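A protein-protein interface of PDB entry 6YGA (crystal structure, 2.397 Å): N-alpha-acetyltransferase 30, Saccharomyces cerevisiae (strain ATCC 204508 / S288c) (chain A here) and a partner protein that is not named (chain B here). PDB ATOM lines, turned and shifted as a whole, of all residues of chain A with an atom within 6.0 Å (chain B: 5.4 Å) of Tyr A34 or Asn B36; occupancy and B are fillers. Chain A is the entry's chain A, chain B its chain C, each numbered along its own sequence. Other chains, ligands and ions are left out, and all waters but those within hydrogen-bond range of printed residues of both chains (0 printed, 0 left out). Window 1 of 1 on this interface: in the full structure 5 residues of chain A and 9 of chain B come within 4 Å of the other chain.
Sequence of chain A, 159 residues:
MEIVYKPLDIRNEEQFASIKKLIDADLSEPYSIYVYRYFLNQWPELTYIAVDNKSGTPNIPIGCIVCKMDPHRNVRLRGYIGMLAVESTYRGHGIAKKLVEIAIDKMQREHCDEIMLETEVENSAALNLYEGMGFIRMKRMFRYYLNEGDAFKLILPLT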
ATOM      1  N   GLU A  13      -5.058  25.016 -11.050  1.00  0.00           N
ATOM      2  CA  GLU A  13      -4.909  24.185  -9.860  1.00  0.00           C
ATOM      3  C   GLU A  13      -6.226  24.051  -9.109  1.00  0.00           C
ATOM      4  O   GLU A  13      -6.509  22.996  -8.530  1.00  0.00           O
ATOM      5  CB  GLU A  13      -3.824  24.764  -8.949  1.00  0.00           C
ATOM      6  CG  GLU A  13      -2.916  23.724  -8.302  1.00  0.00           C
ATOM      7  CD  GLU A  13      -3.548  23.044  -7.100  1.00  0.00           C
ATOM      8  OE1 GLU A  13      -4.421  23.661  -6.456  1.00  0.00           O
ATOM      9  OE2 GLU A  13      -3.167  21.893  -6.802  1.00  0.00           O
ATOM     10  N   SER A  32      -5.867   8.579  -3.831  1.00  0.00           N
ATOM     11  CA  SER A  32      -4.821   9.505  -3.437  1.00  0.00           C
ATOM     12  C   SER A  32      -4.629  10.566  -4.517  1.00  0.00           C
ATOM     13  O   SER A  32      -5.185  10.483  -5.614  1.00  0.00           O
ATOM     14  CB  SER A  32      -3.508   8.766  -3.174  1.00  0.00           C
ATOM     15  OG  SER A  32      -2.922   8.310  -4.382  1.00  0.00           O
ATOM     16  N   ILE A  33      -3.828  11.582  -4.189  1.00  0.00           N
ATOM     17  CA  ILE A  33      -3.512  12.624  -5.164  1.00  0.00           C
ATOM     18  C   ILE A  33      -2.843  12.018  -6.391  1.00  0.00           C
ATOM     19  O   ILE A  33      -3.080  12.450  -7.526  1.00  0.00           O
ATOM     20  CB  ILE A  33      -2.635  13.714  -4.515  1.00  0.00           C
ATOM     21  CG1 ILE A  33      -3.462  14.559  -3.539  1.00  0.00           C
ATOM     22  CG2 ILE A  33      -1.992  14.610  -5.570  1.00  0.00           C
ATOM     23  CD1 ILE A  33      -2.681  15.688  -2.883  1.00  0.00           C
ATOM     24  N   TYR A  34      -2.013  10.995  -6.190  1.00  0.00           N
ATOM     25  CA  TYR A  34      -1.289  10.400  -7.304  1.00  0.00           C
ATOM     26  C   TYR A  34      -2.142   9.448  -8.132  1.00  0.00           C
ATOM     27  O   TYR A  34      -1.737   9.088  -9.242  1.00  0.00           O
ATOM     28  CB  TYR A  34      -0.032   9.702  -6.792  1.00  0.00           C
ATOM     29  CG  TYR A  34       1.122  10.663  -6.684  1.00  0.00           C
ATOM     30  CD1 TYR A  34       1.962  10.887  -7.766  1.00  0.00           C
ATOM     31  CD2 TYR A  34       1.346  11.381  -5.517  1.00  0.00           C
ATOM     32  CE1 TYR A  34       3.012  11.778  -7.683  1.00  0.00           C
ATOM     33  CE2 TYR A  34       2.392  12.275  -5.422  1.00  0.00           C
ATOM     34  CZ  TYR A  34       3.222  12.470  -6.507  1.00  0.00           C
ATOM     35  OH  TYR A  34       4.264  13.362  -6.410  1.00  0.00           O
ATOM     36  N   VAL A  35      -3.313   9.046  -7.638  1.00  0.00           N
ATOM     37  CA  VAL A  35      -4.289   8.409  -8.515  1.00  0.00           C
ATOM     38  C   VAL A  35      -4.803   9.418  -9.534  1.00  0.00           C
ATOM     39  O   VAL A  35      -4.885   9.134 -10.734  1.00  0.00           O
ATOM     40  CB  VAL A  35      -5.442   7.803  -7.696  1.00  0.00           C
ATOM     41  CG1 VAL A  35      -6.442   7.121  -8.618  1.00  0.00           C
ATOM     42  CG2 VAL A  35      -4.913   6.824  -6.666  1.00  0.00           C
ATOM     43  N   TYR A  36      -5.130  10.626  -9.066  1.00  0.00           N
ATOM     44  CA  TYR A  36      -5.602  11.672  -9.969  1.00  0.00           C
ATOM     45  C   TYR A  36      -4.486  12.158 -10.881  1.00  0.00           C
ATOM     46  O   TYR A  36      -4.734  12.522 -12.035  1.00  0.00           O
ATOM     47  CB  TYR A  36      -6.177  12.838  -9.166  1.00  0.00           C
ATOM     48  CG  TYR A  36      -7.441  12.497  -8.415  1.00  0.00           C
ATOM     49  CD1 TYR A  36      -8.674  12.513  -9.052  1.00  0.00           C
ATOM     50  CD2 TYR A  36      -7.402  12.160  -7.069  1.00  0.00           C
ATOM     51  CE1 TYR A  36      -9.834  12.200  -8.371  1.00  0.00           C
ATOM     52  CE2 TYR A  36      -8.557  11.845  -6.378  1.00  0.00           C
ATOM     53  CZ  TYR A  36      -9.771  11.867  -7.035  1.00  0.00           C
ATOM     54  OH  TYR A  36     -10.927  11.556  -6.357  1.00  0.00           O
ATOM     55  N   ARG A  37      -3.251  12.169 -10.382  1.00  0.00           N
ATOM     56  CA  ARG A  37      -2.138  12.644 -11.191  1.00  0.00           C
ATOM     57  C   ARG A  37      -1.754  11.627 -12.259  1.00  0.00           C
ATOM     58  O   ARG A  37      -1.236  12.004 -13.314  1.00  0.00           O
ATOM     59  CB  ARG A  37      -0.952  12.967 -10.290  1.00  0.00           C
ATOM     60  CG  ARG A  37      -0.068  14.059 -10.830  1.00  0.00           C
ATOM     61  CD  ARG A  37       0.426  14.979  -9.731  1.00  0.00           C
ATOM     62  NE  ARG A  37      -0.588  15.939  -9.304  1.00  0.00           N
ATOM     63  CZ  ARG A  37      -0.810  17.104  -9.903  1.00  0.00           C
ATOM     64  NH1 ARG A  37      -0.098  17.451 -10.967  1.00  0.00           N
ATOM     65  NH2 ARG A  37      -1.746  17.923  -9.442  1.00  0.00           N
ATOM     66  N   TYR A  38      -2.005  10.340 -12.004  1.00  0.00           N
ATOM     67  CA  TYR A  38      -1.769   9.319 -13.019  1.00  0.00           C
ATOM     68  C   TYR A  38      -2.687   9.516 -14.219  1.00  0.00           C
ATOM     69  O   TYR A  38      -2.268   9.341 -15.369  1.00  0.00           O
ATOM     70  CB  TYR A  38      -1.965   7.930 -12.410  1.00  0.00           C
ATOM     71  CG  TYR A  38      -2.258   6.832 -13.410  1.00  0.00           C
ATOM     72  CD1 TYR A  38      -1.246   6.276 -14.179  1.00  0.00           C
ATOM     73  CD2 TYR A  38      -3.548   6.339 -13.569  1.00  0.00           C
ATOM     74  CE1 TYR A  38      -1.510   5.267 -15.087  1.00  0.00           C
ATOM     75  CE2 TYR A  38      -3.823   5.332 -14.473  1.00  0.00           C
ATOM     76  CZ  TYR A  38      -2.801   4.800 -15.228  1.00  0.00           C
ATOM     77  OH  TYR A  38      -3.075   3.797 -16.128  1.00  0.00           O
ATOM     78  N   PHE A  39      -3.944   9.889 -13.970  1.00  0.00           N
ATOM     79  CA  PHE A  39      -4.887  10.128 -15.056  1.00  0.00           C
ATOM     80  C   PHE A  39      -4.657  11.486 -15.714  1.00  0.00           C
ATOM     81  O   PHE A  39      -4.464  11.570 -16.931  1.00  0.00           O
ATOM     82  CB  PHE A  39      -6.324  10.038 -14.535  1.00  0.00           C
ATOM     83  CG  PHE A  39      -6.870   8.636 -14.467  1.00  0.00           C
ATOM     84  CD1 PHE A  39      -7.397   8.031 -15.596  1.00  0.00           C
ATOM     85  CD2 PHE A  39      -6.882   7.933 -13.269  1.00  0.00           C
ATOM     86  CE1 PHE A  39      -7.910   6.748 -15.540  1.00  0.00           C
ATOM     87  CE2 PHE A  39      -7.394   6.647 -13.207  1.00  0.00           C
ATOM     88  CZ  PHE A  39      -7.908   6.054 -14.346  1.00  0.00           C
ATOM     89  N   ALA B  30       8.282  10.370  -6.559  1.00  0.00           N
ATOM     90  CA  ALA B  30       7.850  11.408  -7.483  1.00  0.00           C
ATOM     91  C   ALA B  30       7.481  12.663  -6.706  1.00  0.00           C
ATOM     92  O   ALA B  30       7.093  12.597  -5.536  1.00  0.00           O
ATOM     93  CB  ALA B  30       6.664  10.938  -8.336  1.00  0.00           C
ATOM     94  N   VAL B  31       7.615  13.805  -7.376  1.00  0.00           N
ATOM     95  CA  VAL B  31       7.188  15.100  -6.857  1.00  0.00           C
ATOM     96  C   VAL B  31       6.545  15.867  -8.005  1.00  0.00           C
ATOM     97  O   VAL B  31       6.980  15.754  -9.156  1.00  0.00           O
ATOM     98  CB  VAL B  31       8.365  15.888  -6.232  1.00  0.00           C
ATOM     99  CG1 VAL B  31       9.447  16.175  -7.268  1.00  0.00           C
ATOM    100  CG2 VAL B  31       7.876  17.180  -5.586  1.00  0.00           C
ATOM    101  N   ASP B  32       5.489  16.621  -7.703  1.00  0.00           N
ATOM    102  CA  ASP B  32       4.767  17.386  -8.709  1.00  0.00           C
ATOM    103  C   ASP B  32       4.975  18.884  -8.484  1.00  0.00           C
ATOM    104  O   ASP B  32       5.779  19.307  -7.647  1.00  0.00           O
ATOM    105  CB  ASP B  32       3.281  17.008  -8.709  1.00  0.00           C
ATOM    106  CG  ASP B  32       2.578  17.357  -7.407  1.00  0.00           C
ATOM    107  OD1 ASP B  32       3.247  17.827  -6.463  1.00  0.00           O
ATOM    108  OD2 ASP B  32       1.346  17.155  -7.333  1.00  0.00           O
ATOM    109  N   GLN B  34       3.009  21.123  -7.208  1.00  0.00           N
ATOM    110  CA  GLN B  34       2.487  21.627  -5.946  1.00  0.00           C
ATOM    111  C   GLN B  34       3.187  21.016  -4.733  1.00  0.00           C
ATOM    112  O   GLN B  34       2.656  21.094  -3.620  1.00  0.00           O
ATOM    113  CB  GLN B  34       0.979  21.383  -5.873  1.00  0.00           C
ATOM    114  CG  GLN B  34       0.207  21.971  -7.052  1.00  0.00           C
ATOM    115  CD  GLN B  34       0.401  23.475  -7.195  1.00  0.00           C
ATOM    116  OE1 GLN B  34       0.769  23.972  -8.263  1.00  0.00           O
ATOM    117  NE2 GLN B  34       0.146  24.207  -6.118  1.00  0.00           N
ATOM    118  N   MET B  35       4.359  20.418  -4.930  1.00  0.00           N
ATOM    119  CA  MET B  35       5.159  19.807  -3.866  1.00  0.00           C
ATOM    120  C   MET B  35       4.444  18.647  -3.172  1.00  0.00           C
ATOM    121  O   MET B  35       4.714  18.360  -2.006  1.00  0.00           O
ATOM    122  CB  MET B  35       5.582  20.856  -2.828  1.00  0.00           C
ATOM    123  CG  MET B  35       6.956  20.594  -2.221  1.00  0.00           C
ATOM    124  SD  MET B  35       7.436  21.806  -0.768  1.00  0.00           S
ATOM    125  CE  MET B  35       6.286  21.087   0.633  1.00  0.00           C
ATOM    126  N   ASN B  36       3.531  17.983  -3.878  1.00  0.00           N
ATOM    127  CA  ASN B  36       3.014  16.709  -3.394  1.00  0.00           C
ATOM    128  C   ASN B  36       4.070  15.636  -3.616  1.00  0.00           C
ATOM    129  O   ASN B  36       4.592  15.489  -4.725  1.00  0.00           O
ATOM    130  CB  ASN B  36       1.717  16.335  -4.113  1.00  0.00           C
ATOM    131  CG  ASN B  36       0.654  17.410  -4.007  1.00  0.00           C
ATOM    132  OD1 ASN B  36       0.469  18.015  -2.952  1.00  0.00           O
ATOM    133  ND2 ASN B  36      -0.046  17.662  -5.110  1.00  0.00           N
ATOM    134  N   LEU B  37       4.401  14.893  -2.564  1.00  0.00           N
ATOM    135  CA  LEU B  37       5.444  13.881  -2.634  1.00  0.00           C
ATOM    136  C   LEU B  37       4.836  12.487  -2.599  1.00  0.00           C
ATOM    137  O   LEU B  37       3.817  12.257  -1.941  1.00  0.00           O
ATOM    138  CB  LEU B  37       6.441  14.025  -1.482  1.00  0.00           C
ATOM    139  CG  LEU B  37       6.926  15.429  -1.128  1.00  0.00           C
ATOM    140  CD1 LEU B  37       7.621  15.406   0.218  1.00  0.00           C
ATOM    141  CD2 LEU B  37       7.855  15.961  -2.200  1.00  0.00           C
ATOM    142  N   LEU B  38       5.465  11.563  -3.317  1.00  0.00           N
ATOM    143  CA  LEU B  38       5.140  10.146  -3.247  1.00  0.00           C
ATOM    144  C   LEU B  38       6.376   9.405  -2.761  1.00  0.00           C
ATOM    145  O   LEU B  38       7.446   9.517  -3.367  1.00  0.00           O
ATOM    146  CB  LEU B  38       4.687   9.604  -4.608  1.00  0.00           C
ATOM    147  CG  LEU B  38       4.193   8.156  -4.650  1.00  0.00           C
ATOM    148  CD1 LEU B  38       2.927   7.985  -3.824  1.00  0.00           C
ATOM    149  CD2 LEU B  38       3.965   7.705  -6.090  1.00  0.00           C
ATOM    150  N   SER B  57       1.680   8.796  -0.256  1.00  0.00           N
ATOM    151  CA  SER B  57       1.757  10.140  -0.810  1.00  0.00           C
ATOM    152  C   SER B  57       1.435  11.141   0.290  1.00  0.00           C
ATOM    153  O   SER B  57       0.520  10.922   1.087  1.00  0.00           O
ATOM    154  CB  SER B  57       0.789  10.321  -1.986  1.00  0.00           C
ATOM    155  OG  SER B  57      -0.541  10.520  -1.537  1.00  0.00           O
ATOM    156  N   VAL B  58       2.196  12.228   0.344  1.00  0.00           N
ATOM    157  CA  VAL B  58       2.012  13.260   1.354  1.00  0.00           C
ATOM    158  C   VAL B  58       1.617  14.558   0.655  1.00  0.00           C
ATOM    159  O   VAL B  58       2.358  15.054  -0.199  1.00  0.00           O
ATOM    160  CB  VAL B  58       3.265  13.457   2.226  1.00  0.00           C
ATOM    161  CG1 VAL B  58       3.485  12.234   3.101  1.00  0.00           C
ATOM    162  CG2 VAL B  58       4.499  13.705   1.379  1.00  0.00           C
ATOM    163  N   PRO B  59       0.449  15.122   0.950  1.00  0.00           N
ATOM    164  CA  PRO B  59       0.054  16.388   0.324  1.00  0.00           C
ATOM    165  C   PRO B  59       0.875  17.555   0.859  1.00  0.00           C
ATOM    166  O   PRO B  59       1.677  17.425   1.785  1.00  0.00           O
ATOM    167  CB  PRO B  59      -1.427  16.528   0.696  1.00  0.00           C
ATOM    168  CG  PRO B  59      -1.865  15.143   1.089  1.00  0.00           C
ATOM    169  CD  PRO B  59      -0.657  14.510   1.704  1.00  0.00           C
ATOM    170  N   ARG B  60       0.649  18.721   0.251  1.00  0.00           N
ATOM    171  CA  ARG B  60       1.408  19.917   0.609  1.00  0.00           C
ATOM    172  C   ARG B  60       1.174  20.313   2.063  1.00  0.00           C
ATOM    173  O   ARG B  60       2.127  20.534   2.819  1.00  0.00           O
ATOM    174  CB  ARG B  60       1.031  21.067  -0.325  1.00  0.00           C
ATOM    175  CG  ARG B  60       1.373  22.440   0.221  1.00  0.00           C
ATOM    176  CD  ARG B  60       0.772  23.550  -0.626  1.00  0.00           C
ATOM    177  NE  ARG B  60       1.076  24.867  -0.072  1.00  0.00           N
ATOM    178  CZ  ARG B  60       2.214  25.519  -0.286  1.00  0.00           C
ATOM    179  NH1 ARG B  60       3.157  24.975  -1.043  1.00  0.00           N
ATOM    180  NH2 ARG B  60       2.413  26.710   0.258  1.00  0.00           N
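Printed residues of chain B within 4 Å of Ile A33: Asn B36 (3.6 Å) and Pro B59 (3.9 Å). Tyr A34 touches seven residues of chain B. Tyr A36 touches none of the printed residues of chain B. Phe A39 touches none of the printed residues of chain B. Printed residues of chain A within 4 Å of Asp B32: Tyr A34 (3.7 Å) and Arg A37 (3.0 Å). Printed residues of chain A within 4 Å of Gln B34: Glu A13. Asn B36 touches just these residues of chain A: Ile A33 (3.6 Å) and Tyr A34 (2.7 Å). Of the printed residues of chain A, Pro B59 touches Ile A33. The nearest printed residue of chain B that does not touch Tyr A34 is Val B58 (5.8 Å). The nearest residue of chain A that does not touch Asn B36 is Arg A37 (4.6 Å).
OH of Tyr A34 lies within hydrogen-bond range of O of Asn B36 (2.7 Å). NE of Arg A37 lies within salt-bridge range of OD2 of Asp B32 (3.0 Å). The backbone carbonyl oxygen (O) of Ala B30 is in hydrogen-bond range of the side-chain hydroxyl (OH) of Tyr A34 (3.1 Å).
Among the printed residues, merely in contact across the chains: Glu A13 with Gln B34, Ser A32 with Ser B57, Ile A33 with Asn B36, Ile A33 with Pro B59, Tyr A34 with Val B31, Tyr A34 with Asp B32, Tyr A34 with Leu B37, Tyr A34 with Leu B38 and Tyr A34 with Ser B57.
O of Leu B37 is in hydrogen-bond range of N of Val B58 (2.8 Å). The side-chain carboxylate (OD1) of Asp B32 lies within hydrogen-bond range of the backbone NH (N) of Asn B36 (2.6 Å). The side-chain carboxylate of Asp B32 lies close to the backbone NH of Gln B34, 3.4 Å away. The side-chain carboxylate (OD1) of Asp B32 is in hydrogen-bond range of the backbone NH (N) of Met B35, at 3.2 Å. The backbone NH (N) of Leu B38 sits at hydrogen-bond distance from the backbone carbonyl oxygen (O) of Ala B30, at 2.9 Å. The backbone NH of Arg B60 lies within hydrogen-bond range of the side-chain amide oxygen of Asn B36, 3.3 Å away.
Of the 9 printed residues of chain A, 5 touch a printed residue of chain B. Hydrophobic or aromatic side chains of chain A within 4 Å of the printed part of chain B: Ile A33 and Tyr A34. Of the 12 printed residues of chain B, 9 touch a printed residue of chain A. Among the printed residues, 12 pairs touch across the chains. Among the printed residues, Asp or Glu carboxylates within 4 Å of a Lys or Arg side-chain nitrogen of the other chain: Arg A37 with Asp B32.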
